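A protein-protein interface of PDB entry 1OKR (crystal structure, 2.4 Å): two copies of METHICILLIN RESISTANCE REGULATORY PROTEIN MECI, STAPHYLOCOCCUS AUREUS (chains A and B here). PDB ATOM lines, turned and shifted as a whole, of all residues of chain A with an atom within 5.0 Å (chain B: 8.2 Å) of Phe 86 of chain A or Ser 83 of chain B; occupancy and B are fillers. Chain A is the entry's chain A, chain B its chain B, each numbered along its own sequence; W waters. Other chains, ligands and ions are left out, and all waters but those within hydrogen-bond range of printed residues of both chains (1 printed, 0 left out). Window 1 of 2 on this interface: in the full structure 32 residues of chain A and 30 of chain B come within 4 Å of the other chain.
OG of Ser 83 of chain A is in hydrogen-bond range of OH of Tyr 91 of chain B (2.5 Å).
The backbone carbonyl oxygen (O) of Lys 79 of chain B lies within hydrogen-bond range of the side-chain hydroxyl (OH) of Tyr 91 of chain A (3.0 Å).
The side-chain hydroxyl (OH) of Tyr 91 of chain A is in hydrogen-bond range of the side-chain hydroxyl (OG) of Ser 83 of chain B (2.8 Å).
ND2 of Asn 101 of chain A is in hydrogen-bond range of O of Ser 76 of chain B, at 3.1 Å.
The side-chain amide oxygen (OD1) of Asn 101 of chain A lies close to the backbone NH (N) of Tyr 80 of chain B, 3.4 Å away.
OD1 of Asn 101 of chain A lies within hydrogen-bond range of OH of Tyr 91 of chain A (3.1 Å).
O of Ile 8 of chain B is in hydrogen-bond range of NE1 of Trp 13 of chain B (3.3 Å).
The backbone carbonyl oxygen of Ile 78 of chain B is in hydrogen-bond range of the side-chain hydroxyl of Thr 82 of chain B (2.5 Å).
The backbone carbonyl oxygen (O) of Lys 79 of chain B is in hydrogen-bond range of the side-chain hydroxyl (OG) of Ser 83 of chain B (3.1 Å).
Among the printed residues, pairs that only touch across the chains: Val 90 of chain A with Lys 79 of chain B, Phe 86 of chain A with Phe 86 of chain B, Lys 89 of chain A with Trp 13 of chain B, Phe 86 of chain A with Ser 83 of chain B, Lys 89 of chain A with Ser 10 of chain B, Leu 98 of chain A with Phe 95 of chain B, Val 90 of chain A with Trp 13 of chain B, Thr 82 of chain A with Phe 86 of chain B, Phe 86 of chain A with Thr 82 of chain B, Asn 101 of chain A with Lys 79 of chain B and Ser 83 of chain A with Phe 86 of chain B.
Phe 86 of chain A touches just these residues of chain B: Thr 82 (3.8 Å), Ser 83 (3.7 Å) and Phe 86 (3.4 Å).
Ser 83 of chain B touches two residues of chain A.
Of the printed residues of chain A, Ser 76 of chain B touches Asn 101.
Of the printed residues of chain B, Thr 82 of chain A touches Phe 86 (3.8 Å).
Asn 88 of chain B touches none of the printed residues of chain A.
The nearest residue of chain A that does not touch Ser 83 of chain B is Leu 98 of chain A (4.2 Å).
Of the 12 printed residues of chain A, 8 touch a printed residue of chain B.
Printed residues of chain A that touch a printed residue of chain B: Thr 82, Ser 83, Phe 86, Lys 89, Val 90, Tyr 91, Leu 98 and Asn 101.
Printed residues of chain B that touch a printed residue of chain A: Ser 10, Trp 13, Ser 76, Lys 79, Tyr 80, Thr 82, Ser 83, Phe 86, Tyr 91 and Phe 95.
Among the printed residues, 16 pairs touch across the chains.
Among the printed residues, no Asp or Glu carboxylate lies within 4 Å of a Lys or Arg side-chain nitrogen of the other chain.
Thr 82 of chain A touches Phe 86 of chain B, and with the chains exchanged Phe 86 of chain A touches Thr 82 of chain B.
Ser 83 of chain A touches Phe 86 of chain B, and with the chains exchanged Phe 86 of chain A touches Ser 83 of chain B.
Ser 83 of chain A touches Tyr 91 of chain B, and with the chains exchanged Tyr 91 of chain A touches Ser 83 of chain B.
Phe 86 of chain A touches its own counterpart, Phe 86 of chain B.
Positions printed for both chains: 82, 83, 84, 85, 86, 87, 88, 89, 90, 91 and 98.
Water W1 bridges the backbone carbonyl oxygen of Ile 8 of chain B (2.6 Å) and the side-chain amino group of Lys 89 of chain A (3.3 Å).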
ATOM      1  N   THR A  82      -5.335 -17.787 -26.418  1.00  0.00           N
ATOM      2  CA  THR A  82      -4.119 -17.416 -25.723  1.00  0.00           C
ATOM      3  C   THR A  82      -3.004 -18.511 -25.821  1.00  0.00           C
ATOM      4  O   THR A  82      -1.837 -18.229 -26.212  1.00  0.00           O
ATOM      5  CB  THR A  82      -4.438 -17.078 -24.272  1.00  0.00           C
ATOM      6  OG1 THR A  82      -5.504 -16.095 -24.184  1.00  0.00           O
ATOM      7  CG2 THR A  82      -3.211 -16.393 -23.604  1.00  0.00           C
ATOM      8  N   SER A  83      -3.367 -19.755 -25.503  1.00  0.00           N
ATOM      9  CA  SER A  83      -2.430 -20.875 -25.590  1.00  0.00           C
ATOM     10  C   SER A  83      -1.870 -21.003 -26.987  1.00  0.00           C
ATOM     11  O   SER A  83      -0.747 -21.422 -27.176  1.00  0.00           O
ATOM     12  CB  SER A  83      -3.077 -22.197 -25.209  1.00  0.00           C
ATOM     13  OG  SER A  83      -3.494 -22.229 -23.840  1.00  0.00           O
ATOM     14  N   LYS A  84      -2.647 -20.653 -27.980  1.00  0.00           N
ATOM     15  CA  LYS A  84      -2.191 -20.820 -29.359  1.00  0.00           C
ATOM     16  C   LYS A  84      -1.188 -19.739 -29.701  1.00  0.00           C
ATOM     17  O   LYS A  84      -0.199 -20.012 -30.363  1.00  0.00           O
ATOM     18  CB  LYS A  84      -3.371 -20.798 -30.339  1.00  0.00           C
ATOM     19  CG  LYS A  84      -4.041 -22.164 -30.540  1.00  0.00           C
ATOM     20  CD  LYS A  84      -4.374 -22.385 -32.039  1.00  0.00           C
ATOM     21  CE  LYS A  84      -3.124 -22.734 -32.881  1.00  0.00           C
ATOM     22  NZ  LYS A  84      -3.131 -24.155 -33.389  1.00  0.00           N
ATOM     23  N   ASN A  85      -1.426 -18.516 -29.245  1.00  0.00           N
ATOM     24  CA  ASN A  85      -0.457 -17.446 -29.477  1.00  0.00           C
ATOM     25  C   ASN A  85       0.865 -17.742 -28.794  1.00  0.00           C
ATOM     26  O   ASN A  85       1.921 -17.546 -29.394  1.00  0.00           O
ATOM     27  CB  ASN A  85      -1.008 -16.077 -29.055  1.00  0.00           C
ATOM     28  CG  ASN A  85      -2.151 -15.577 -29.992  1.00  0.00           C
ATOM     29  OD1 ASN A  85      -2.864 -14.629 -29.674  1.00  0.00           O
ATOM     30  ND2 ASN A  85      -2.322 -16.240 -31.121  1.00  0.00           N
ATOM     31  N   PHE A  86       0.782 -18.231 -27.560  1.00  0.00           N
ATOM     32  CA  PHE A  86       1.910 -18.673 -26.768  1.00  0.00           C
ATOM     33  C   PHE A  86       2.752 -19.785 -27.417  1.00  0.00           C
ATOM     34  O   PHE A  86       3.982 -19.715 -27.450  1.00  0.00           O
ATOM     35  CB  PHE A  86       1.391 -19.195 -25.417  1.00  0.00           C
ATOM     36  CG  PHE A  86       2.495 -19.661 -24.491  1.00  0.00           C
ATOM     37  CD1 PHE A  86       3.262 -18.758 -23.788  1.00  0.00           C
ATOM     38  CD2 PHE A  86       2.804 -20.990 -24.370  1.00  0.00           C
ATOM     39  CE1 PHE A  86       4.292 -19.198 -22.947  1.00  0.00           C
ATOM     40  CE2 PHE A  86       3.833 -21.418 -23.538  1.00  0.00           C
ATOM     41  CZ  PHE A  86       4.568 -20.503 -22.836  1.00  0.00           C
ATOM     42  N   ILE A  87       2.096 -20.829 -27.897  1.00  0.00           N
ATOM     43  CA  ILE A  87       2.782 -21.941 -28.566  1.00  0.00           C
ATOM     44  C   ILE A  87       3.424 -21.459 -29.858  1.00  0.00           C
ATOM     45  O   ILE A  87       4.483 -21.924 -30.195  1.00  0.00           O
ATOM     46  CB  ILE A  87       1.794 -23.131 -28.842  1.00  0.00           C
ATOM     47  CG1 ILE A  87       1.362 -23.790 -27.541  1.00  0.00           C
ATOM     48  CG2 ILE A  87       2.405 -24.229 -29.746  1.00  0.00           C
ATOM     49  CD1 ILE A  87       0.029 -24.489 -27.670  1.00  0.00           C
ATOM     50  N   ASN A  88       2.813 -20.521 -30.575  1.00  0.00           N
ATOM     51  CA  ASN A  88       3.433 -19.999 -31.804  1.00  0.00           C
ATOM     52  C   ASN A  88       4.651 -19.148 -31.445  1.00  0.00           C
ATOM     53  O   ASN A  88       5.656 -19.177 -32.140  1.00  0.00           O
ATOM     54  CB  ASN A  88       2.443 -19.144 -32.641  1.00  0.00           C
ATOM     55  CG  ASN A  88       1.498 -19.982 -33.516  1.00  0.00           C
ATOM     56  OD1 ASN A  88       0.979 -19.477 -34.513  1.00  0.00           O
ATOM     57  ND2 ASN A  88       1.263 -21.256 -33.145  1.00  0.00           N
ATOM     58  N   LYS A  89       4.540 -18.395 -30.351  1.00  0.00           N
ATOM     59  CA  LYS A  89       5.578 -17.485 -29.904  1.00  0.00           C
ATOM     60  C   LYS A  89       6.828 -18.218 -29.420  1.00  0.00           C
ATOM     61  O   LYS A  89       7.926 -17.829 -29.777  1.00  0.00           O
ATOM     62  CB  LYS A  89       5.051 -16.625 -28.740  1.00  0.00           C
ATOM     63  CG  LYS A  89       6.108 -15.782 -28.095  1.00  0.00           C
ATOM     64  CD  LYS A  89       5.601 -14.858 -27.051  1.00  0.00           C
ATOM     65  CE  LYS A  89       5.572 -15.471 -25.698  1.00  0.00           C
ATOM     66  NZ  LYS A  89       4.660 -14.701 -24.783  1.00  0.00           N
ATOM     67  N   VAL A  90       6.647 -19.250 -28.588  1.00  0.00           N
ATOM     68  CA  VAL A  90       7.773 -19.968 -27.952  1.00  0.00           C
ATOM     69  C   VAL A  90       8.307 -21.235 -28.667  1.00  0.00           C
ATOM     70  O   VAL A  90       9.542 -21.456 -28.783  1.00  0.00           O
ATOM     71  CB  VAL A  90       7.376 -20.345 -26.542  1.00  0.00           C
ATOM     72  CG1 VAL A  90       8.422 -21.209 -25.863  1.00  0.00           C
ATOM     73  CG2 VAL A  90       7.176 -19.126 -25.787  1.00  0.00           C
ATOM     74  N   TYR A  91       7.376 -22.063 -29.142  1.00  0.00           N
ATOM     75  CA  TYR A  91       7.716 -23.399 -29.616  1.00  0.00           C
ATOM     76  C   TYR A  91       7.560 -23.603 -31.098  1.00  0.00           C
ATOM     77  O   TYR A  91       7.098 -24.650 -31.499  1.00  0.00           O
ATOM     78  CB  TYR A  91       6.808 -24.410 -28.932  1.00  0.00           C
ATOM     79  CG  TYR A  91       7.071 -24.609 -27.472  1.00  0.00           C
ATOM     80  CD1 TYR A  91       8.060 -25.492 -27.050  1.00  0.00           C
ATOM     81  CD2 TYR A  91       6.322 -23.962 -26.514  1.00  0.00           C
ATOM     82  CE1 TYR A  91       8.305 -25.711 -25.754  1.00  0.00           C
ATOM     83  CE2 TYR A  91       6.577 -24.184 -25.152  1.00  0.00           C
ATOM     84  CZ  TYR A  91       7.571 -25.059 -24.800  1.00  0.00           C
ATOM     85  OH  TYR A  91       7.861 -25.325 -23.504  1.00  0.00           O
ATOM     86  N   LEU A  98       5.647 -28.564 -27.088  1.00  0.00           N
ATOM     87  CA  LEU A  98       5.339 -28.086 -25.756  1.00  0.00           C
ATOM     88  C   LEU A  98       5.223 -29.249 -24.824  1.00  0.00           C
ATOM     89  O   LEU A  98       5.781 -29.221 -23.754  1.00  0.00           O
ATOM     90  CB  LEU A  98       3.995 -27.344 -25.707  1.00  0.00           C
ATOM     91  CG  LEU A  98       3.708 -26.619 -24.386  1.00  0.00           C
ATOM     92  CD1 LEU A  98       3.021 -25.319 -24.699  1.00  0.00           C
ATOM     93  CD2 LEU A  98       2.866 -27.432 -23.431  1.00  0.00           C
ATOM     94  N   ASN A 101       8.489 -31.075 -24.230  1.00  0.00           N
ATOM     95  CA  ASN A 101       9.285 -30.273 -23.293  1.00  0.00           C
ATOM     96  C   ASN A 101       8.812 -30.497 -21.857  1.00  0.00           C
ATOM     97  O   ASN A 101       9.614 -30.785 -20.962  1.00  0.00           O
ATOM     98  CB  ASN A 101       9.249 -28.791 -23.669  1.00  0.00           C
ATOM     99  CG  ASN A 101      10.024 -27.922 -22.717  1.00  0.00           C
ATOM    100  OD1 ASN A 101       9.441 -27.330 -21.829  1.00  0.00           O
ATOM    101  ND2 ASN A 101      11.333 -27.816 -22.906  1.00  0.00           N
ATOM    102  N   GLU B   7      11.464 -11.485 -18.432  1.00  0.00           N
ATOM    103  CA  GLU B   7      10.580 -12.004 -19.465  1.00  0.00           C
ATOM    104  C   GLU B   7      11.271 -11.771 -20.812  1.00  0.00           C
ATOM    105  O   GLU B   7      12.179 -10.929 -20.938  1.00  0.00           O
ATOM    106  CB  GLU B   7       9.242 -11.249 -19.429  1.00  0.00           C
ATOM    107  CG  GLU B   7       7.976 -12.115 -19.414  1.00  0.00           C
ATOM    108  CD  GLU B   7       7.926 -13.147 -18.302  1.00  0.00           C
ATOM    109  OE1 GLU B   7       7.558 -14.302 -18.596  1.00  0.00           O
ATOM    110  OE2 GLU B   7       8.238 -12.820 -17.150  1.00  0.00           O
ATOM    111  N   ILE B   8      10.838 -12.548 -21.790  1.00  0.00           N
ATOM    112  CA  ILE B   8      11.359 -12.535 -23.127  1.00  0.00           C
ATOM    113  C   ILE B   8      10.188 -12.232 -24.012  1.00  0.00           C
ATOM    114  O   ILE B   8       9.180 -12.891 -23.955  1.00  0.00           O
ATOM    115  CB  ILE B   8      11.892 -13.938 -23.473  1.00  0.00           C
ATOM    116  CG1 ILE B   8      12.590 -14.544 -22.252  1.00  0.00           C
ATOM    117  CG2 ILE B   8      12.853 -13.910 -24.717  1.00  0.00           C
ATOM    118  CD1 ILE B   8      13.500 -15.753 -22.590  1.00  0.00           C
ATOM    119  N   SER B  10       8.120 -11.741 -27.611  1.00  0.00           N
ATOM    120  CA  SER B  10       7.930 -12.507 -28.810  1.00  0.00           C
ATOM    121  C   SER B  10       9.050 -12.319 -29.829  1.00  0.00           C
ATOM    122  O   SER B  10       9.499 -13.260 -30.470  1.00  0.00           O
ATOM    123  CB  SER B  10       6.630 -12.067 -29.450  1.00  0.00           C
ATOM    124  OG  SER B  10       6.427 -12.884 -30.545  1.00  0.00           O
ATOM    125  N   TRP B  13      12.194 -13.992 -28.780  1.00  0.00           N
ATOM    126  CA  TRP B  13      12.152 -15.432 -28.990  1.00  0.00           C
ATOM    127  C   TRP B  13      12.565 -15.798 -30.414  1.00  0.00           C
ATOM    128  O   TRP B  13      13.179 -16.839 -30.628  1.00  0.00           O
ATOM    129  CB  TRP B  13      10.788 -15.992 -28.683  1.00  0.00           C
ATOM    130  CG  TRP B  13      10.461 -16.193 -27.217  1.00  0.00           C
ATOM    131  CD1 TRP B  13       9.576 -15.485 -26.480  1.00  0.00           C
ATOM    132  CD2 TRP B  13      10.950 -17.230 -26.352  1.00  0.00           C
ATOM    133  NE1 TRP B  13       9.501 -15.982 -25.201  1.00  0.00           N
ATOM    134  CE2 TRP B  13      10.319 -17.068 -25.103  1.00  0.00           C
ATOM    135  CE3 TRP B  13      11.878 -18.265 -26.497  1.00  0.00           C
ATOM    136  CZ2 TRP B  13      10.608 -17.884 -24.003  1.00  0.00           C
ATOM    137  CZ3 TRP B  13      12.134 -19.084 -25.423  1.00  0.00           C
ATOM    138  CH2 TRP B  13      11.504 -18.885 -24.189  1.00  0.00           C
ATOM    139  N   SER B  76      15.798 -25.855 -23.304  1.00  0.00           N
ATOM    140  CA  SER B  76      14.701 -26.667 -22.807  1.00  0.00           C
ATOM    141  C   SER B  76      14.371 -26.241 -21.390  1.00  0.00           C
ATOM    142  O   SER B  76      13.242 -26.299 -20.958  1.00  0.00           O
ATOM    143  CB  SER B  76      15.129 -28.140 -22.797  1.00  0.00           C
ATOM    144  OG  SER B  76      16.377 -28.288 -22.115  1.00  0.00           O
ATOM    145  N   ASP B  77      15.372 -25.828 -20.652  1.00  0.00           N
ATOM    146  CA  ASP B  77      15.128 -25.293 -19.329  1.00  0.00           C
ATOM    147  C   ASP B  77      14.318 -23.992 -19.382  1.00  0.00           C
ATOM    148  O   ASP B  77      13.335 -23.838 -18.640  1.00  0.00           O
ATOM    149  CB  ASP B  77      16.450 -25.045 -18.580  1.00  0.00           C
ATOM    150  CG  ASP B  77      17.170 -26.334 -18.229  1.00  0.00           C
ATOM    151  OD1 ASP B  77      16.485 -27.352 -17.994  1.00  0.00           O
ATOM    152  OD2 ASP B  77      18.423 -26.428 -18.154  1.00  0.00           O
ATOM    153  N   ILE B  78      14.734 -23.065 -20.239  1.00  0.00           N
ATOM    154  CA  ILE B  78      14.114 -21.738 -20.318  1.00  0.00           C
ATOM    155  C   ILE B  78      12.665 -21.807 -20.882  1.00  0.00           C
ATOM    156  O   ILE B  78      11.752 -21.146 -20.374  1.00  0.00           O
ATOM    157  CB  ILE B  78      15.062 -20.729 -21.094  1.00  0.00           C
ATOM    158  CG1 ILE B  78      14.508 -19.286 -21.107  1.00  0.00           C
ATOM    159  CG2 ILE B  78      15.331 -21.151 -22.539  1.00  0.00           C
ATOM    160  CD1 ILE B  78      14.185 -18.706 -19.720  1.00  0.00           C
ATOM    161  N   LYS B  79      12.460 -22.637 -21.903  1.00  0.00           N
ATOM    162  CA  LYS B  79      11.148 -22.860 -22.460  1.00  0.00           C
ATOM    163  C   LYS B  79      10.209 -23.582 -21.462  1.00  0.00           C
ATOM    164  O   LYS B  79       9.011 -23.354 -21.489  1.00  0.00           O
ATOM    165  CB  LYS B  79      11.250 -23.667 -23.757  1.00  0.00           C
ATOM    166  CG  LYS B  79      11.771 -22.830 -24.910  1.00  0.00           C
ATOM    167  CD  LYS B  79      12.000 -23.648 -26.186  1.00  0.00           C
ATOM    168  CE  LYS B  79      12.163 -22.719 -27.386  1.00  0.00           C
ATOM    169  NZ  LYS B  79      12.434 -23.449 -28.678  1.00  0.00           N
ATOM    170  N   TYR B  80      10.748 -24.465 -20.611  1.00  0.00           N
ATOM    171  CA  TYR B  80       9.945 -25.141 -19.591  1.00  0.00           C
ATOM    172  C   TYR B  80       9.468 -24.153 -18.528  1.00  0.00           C
ATOM    173  O   TYR B  80       8.294 -24.037 -18.293  1.00  0.00           O
ATOM    174  CB  TYR B  80      10.758 -26.247 -18.940  1.00  0.00           C
ATOM    175  CG  TYR B  80      10.105 -26.924 -17.724  1.00  0.00           C
ATOM    176  CD1 TYR B  80       8.999 -27.741 -17.862  1.00  0.00           C
ATOM    177  CD2 TYR B  80      10.646 -26.767 -16.429  1.00  0.00           C
ATOM    178  CE1 TYR B  80       8.445 -28.383 -16.746  1.00  0.00           C
ATOM    179  CE2 TYR B  80      10.101 -27.395 -15.329  1.00  0.00           C
ATOM    180  CZ  TYR B  80       9.006 -28.216 -15.496  1.00  0.00           C
ATOM    181  OH  TYR B  80       8.455 -28.842 -14.398  1.00  0.00           O
ATOM    182  N   LYS B  81      10.398 -23.417 -17.945  1.00  0.00           N
ATOM    183  CA  LYS B  81      10.115 -22.371 -17.005  1.00  0.00           C
ATOM    184  C   LYS B  81       9.081 -21.418 -17.584  1.00  0.00           C
ATOM    185  O   LYS B  81       8.128 -21.056 -16.894  1.00  0.00           O
ATOM    186  CB  LYS B  81      11.425 -21.628 -16.651  1.00  0.00           C
ATOM    187  CG  LYS B  81      11.337 -20.647 -15.467  1.00  0.00           C
ATOM    188  CD  LYS B  81      12.394 -19.496 -15.538  1.00  0.00           C
ATOM    189  CE  LYS B  81      12.584 -18.756 -14.164  1.00  0.00           C
ATOM    190  NZ  LYS B  81      11.886 -17.422 -14.036  1.00  0.00           N
ATOM    191  N   THR B  82       9.268 -20.997 -18.837  1.00  0.00           N
ATOM    192  CA  THR B  82       8.332 -20.055 -19.472  1.00  0.00           C
ATOM    193  C   THR B  82       6.923 -20.696 -19.557  1.00  0.00           C
ATOM    194  O   THR B  82       5.888 -20.086 -19.256  1.00  0.00           O
ATOM    195  CB  THR B  82       8.798 -19.757 -20.853  1.00  0.00           C
ATOM    196  OG1 THR B  82      10.143 -19.263 -20.833  1.00  0.00           O
ATOM    197  CG2 THR B  82       7.971 -18.643 -21.478  1.00  0.00           C
ATOM    198  N   SER B  83       6.900 -21.962 -19.949  1.00  0.00           N
ATOM    199  CA  SER B  83       5.664 -22.738 -19.962  1.00  0.00           C
ATOM    200  C   SER B  83       5.012 -22.852 -18.581  1.00  0.00           C
ATOM    201  O   SER B  83       3.834 -22.643 -18.462  1.00  0.00           O
ATOM    202  CB  SER B  83       5.921 -24.116 -20.557  1.00  0.00           C
ATOM    203  OG  SER B  83       5.985 -24.016 -21.938  1.00  0.00           O
ATOM    204  N   LYS B  84       5.777 -23.157 -17.545  1.00  0.00           N
ATOM    205  CA  LYS B  84       5.230 -23.196 -16.188  1.00  0.00           C
ATOM    206  C   LYS B  84       4.638 -21.875 -15.691  1.00  0.00           C
ATOM    207  O   LYS B  84       3.528 -21.884 -15.166  1.00  0.00           O
ATOM    208  CB  LYS B  84       6.220 -23.801 -15.152  1.00  0.00           C
ATOM    209  CG  LYS B  84       6.002 -25.365 -15.043  1.00  0.00           C
ATOM    210  CD  LYS B  84       6.489 -26.001 -13.713  1.00  0.00           C
ATOM    211  CE  LYS B  84       5.368 -26.536 -12.772  1.00  0.00           C
ATOM    212  NZ  LYS B  84       4.135 -27.067 -13.443  1.00  0.00           N
ATOM    213  N   ASN B  85       5.338 -20.755 -15.860  1.00  0.00           N
ATOM    214  CA  ASN B  85       4.756 -19.472 -15.526  1.00  0.00           C
ATOM    215  C   ASN B  85       3.436 -19.203 -16.267  1.00  0.00           C
ATOM    216  O   ASN B  85       2.472 -18.686 -15.663  1.00  0.00           O
ATOM    217  CB  ASN B  85       5.693 -18.328 -15.838  1.00  0.00           C
ATOM    218  CG  ASN B  85       6.994 -18.423 -15.104  1.00  0.00           C
ATOM    219  OD1 ASN B  85       8.005 -17.913 -15.582  1.00  0.00           O
ATOM    220  ND2 ASN B  85       6.991 -19.082 -13.950  1.00  0.00           N
ATOM    221  N   PHE B  86       3.393 -19.571 -17.556  1.00  0.00           N
ATOM    222  CA  PHE B  86       2.259 -19.268 -18.417  1.00  0.00           C
ATOM    223  C   PHE B  86       1.092 -20.106 -18.010  1.00  0.00           C
ATOM    224  O   PHE B  86      -0.048 -19.646 -18.087  1.00  0.00           O
ATOM    225  CB  PHE B  86       2.595 -19.511 -19.896  1.00  0.00           C
ATOM    226  CG  PHE B  86       1.406 -19.437 -20.798  1.00  0.00           C
ATOM    227  CD1 PHE B  86       0.980 -18.215 -21.301  1.00  0.00           C
ATOM    228  CD2 PHE B  86       0.677 -20.600 -21.119  1.00  0.00           C
ATOM    229  CE1 PHE B  86      -0.151 -18.135 -22.105  1.00  0.00           C
ATOM    230  CE2 PHE B  86      -0.461 -20.534 -21.914  1.00  0.00           C
ATOM    231  CZ  PHE B  86      -0.861 -19.307 -22.423  1.00  0.00           C
ATOM    232  N   ILE B  87       1.369 -21.354 -17.606  1.00  0.00           N
ATOM    233  CA  ILE B  87       0.325 -22.267 -17.093  1.00  0.00           C
ATOM    234  C   ILE B  87      -0.186 -21.757 -15.744  1.00  0.00           C
ATOM    235  O   ILE B  87      -1.348 -21.751 -15.502  1.00  0.00           O
ATOM    236  CB  ILE B  87       0.881 -23.738 -16.966  1.00  0.00           C
ATOM    237  CG1 ILE B  87       1.020 -24.373 -18.341  1.00  0.00           C
ATOM    238  CG2 ILE B  87      -0.010 -24.611 -16.069  1.00  0.00           C
ATOM    239  CD1 ILE B  87       1.835 -25.596 -18.327  1.00  0.00           C
ATOM    240  N   ASN B  88       0.695 -21.321 -14.873  1.00  0.00           N
ATOM    241  CA  ASN B  88       0.279 -20.717 -13.612  1.00  0.00           C
ATOM    242  C   ASN B  88      -0.509 -19.385 -13.782  1.00  0.00           C
ATOM    243  O   ASN B  88      -1.382 -19.057 -12.978  1.00  0.00           O
ATOM    244  CB  ASN B  88       1.493 -20.583 -12.656  1.00  0.00           C
ATOM    245  CG  ASN B  88       1.851 -21.956 -11.947  1.00  0.00           C
ATOM    246  OD1 ASN B  88       1.557 -22.136 -10.757  1.00  0.00           O
ATOM    247  ND2 ASN B  88       2.453 -22.919 -12.705  1.00  0.00           N
ATOM    248  N   LYS B  89      -0.262 -18.663 -14.862  1.00  0.00           N
ATOM    249  CA  LYS B  89      -0.933 -17.380 -15.073  1.00  0.00           C
ATOM    250  C   LYS B  89      -2.365 -17.641 -15.618  1.00  0.00           C
ATOM    251  O   LYS B  89      -3.368 -17.065 -15.125  1.00  0.00           O
ATOM    252  CB  LYS B  89      -0.123 -16.531 -16.049  1.00  0.00           C
ATOM    253  CG  LYS B  89      -0.926 -15.490 -16.786  1.00  0.00           C
ATOM    254  CD  LYS B  89       0.010 -14.551 -17.571  1.00  0.00           C
ATOM    255  CE  LYS B  89       0.386 -15.114 -18.924  1.00  0.00           C
ATOM    256  NZ  LYS B  89      -0.246 -14.288 -19.947  1.00  0.00           N
ATOM    257  N   VAL B  90      -2.456 -18.561 -16.589  1.00  0.00           N
ATOM    258  CA  VAL B  90      -3.692 -18.732 -17.335  1.00  0.00           C
ATOM    259  C   VAL B  90      -4.508 -19.851 -16.787  1.00  0.00           C
ATOM    260  O   VAL B  90      -5.729 -19.702 -16.701  1.00  0.00           O
ATOM    261  CB  VAL B  90      -3.453 -18.906 -18.846  1.00  0.00           C
ATOM    262  CG1 VAL B  90      -4.741 -19.112 -19.612  1.00  0.00           C
ATOM    263  CG2 VAL B  90      -2.762 -17.732 -19.366  1.00  0.00           C
ATOM    264  N   TYR B  91      -3.858 -20.953 -16.402  1.00  0.00           N
ATOM    265  CA  TYR B  91      -4.586 -22.210 -16.133  1.00  0.00           C
ATOM    266  C   TYR B  91      -4.728 -22.618 -14.661  1.00  0.00           C
ATOM    267  O   TYR B  91      -5.114 -23.743 -14.369  1.00  0.00           O
ATOM    268  CB  TYR B  91      -4.017 -23.382 -16.976  1.00  0.00           C
ATOM    269  CG  TYR B  91      -4.398 -23.282 -18.430  1.00  0.00           C
ATOM    270  CD1 TYR B  91      -5.652 -23.644 -18.869  1.00  0.00           C
ATOM    271  CD2 TYR B  91      -3.512 -22.789 -19.361  1.00  0.00           C
ATOM    272  CE1 TYR B  91      -6.019 -23.521 -20.207  1.00  0.00           C
ATOM    273  CE2 TYR B  91      -3.863 -22.680 -20.698  1.00  0.00           C
ATOM    274  CZ  TYR B  91      -5.119 -23.036 -21.112  1.00  0.00           C
ATOM    275  OH  TYR B  91      -5.467 -22.904 -22.433  1.00  0.00           O
ATOM    276  N   GLY B  93      -2.367 -23.296 -12.831  1.00  0.00           N
ATOM    277  CA  GLY B  93      -1.258 -24.196 -12.560  1.00  0.00           C
ATOM    278  C   GLY B  93      -1.423 -25.629 -13.089  1.00  0.00           C
ATOM    279  O   GLY B  93      -0.484 -26.429 -12.956  1.00  0.00           O
ATOM    280  N   PHE B  95      -1.252 -27.939 -15.914  1.00  0.00           N
ATOM    281  CA  PHE B  95      -0.874 -28.470 -17.224  1.00  0.00           C
ATOM    282  C   PHE B  95      -1.963 -29.375 -17.825  1.00  0.00           C
ATOM    283  O   PHE B  95      -2.270 -29.304 -19.005  1.00  0.00           O
ATOM    284  CB  PHE B  95       0.385 -29.318 -17.094  1.00  0.00           C
ATOM    285  CG  PHE B  95       0.835 -29.939 -18.396  1.00  0.00           C
ATOM    286  CD1 PHE B  95       1.271 -29.128 -19.451  1.00  0.00           C
ATOM    287  CD2 PHE B  95       0.860 -31.324 -18.553  1.00  0.00           C
ATOM    288  CE1 PHE B  95       1.699 -29.674 -20.644  1.00  0.00           C
ATOM    289  CE2 PHE B  95       1.281 -31.891 -19.730  1.00  0.00           C
ATOM    290  CZ  PHE B  95       1.704 -31.074 -20.789  1.00  0.00           C
ATOM    291  N   LEU B  98      -4.512 -27.189 -19.523  1.00  0.00           N
ATOM    292  CA  LEU B  98      -4.079 -26.714 -20.813  1.00  0.00           C
ATOM    293  C   LEU B  98      -4.285 -27.803 -21.866  1.00  0.00           C
ATOM    294  O   LEU B  98      -4.840 -27.559 -22.911  1.00  0.00           O
ATOM    295  CB  LEU B  98      -2.615 -26.306 -20.731  1.00  0.00           C
ATOM    296  CG  LEU B  98      -2.029 -25.632 -21.993  1.00  0.00           C
ATOM    297  CD1 LEU B  98      -0.687 -25.009 -21.662  1.00  0.00           C
ATOM    298  CD2 LEU B  98      -1.843 -26.635 -23.090  1.00  0.00           C
HETATM  299  O   HOH W   1       6.659 -12.552 -23.359  1.00  0.00           O
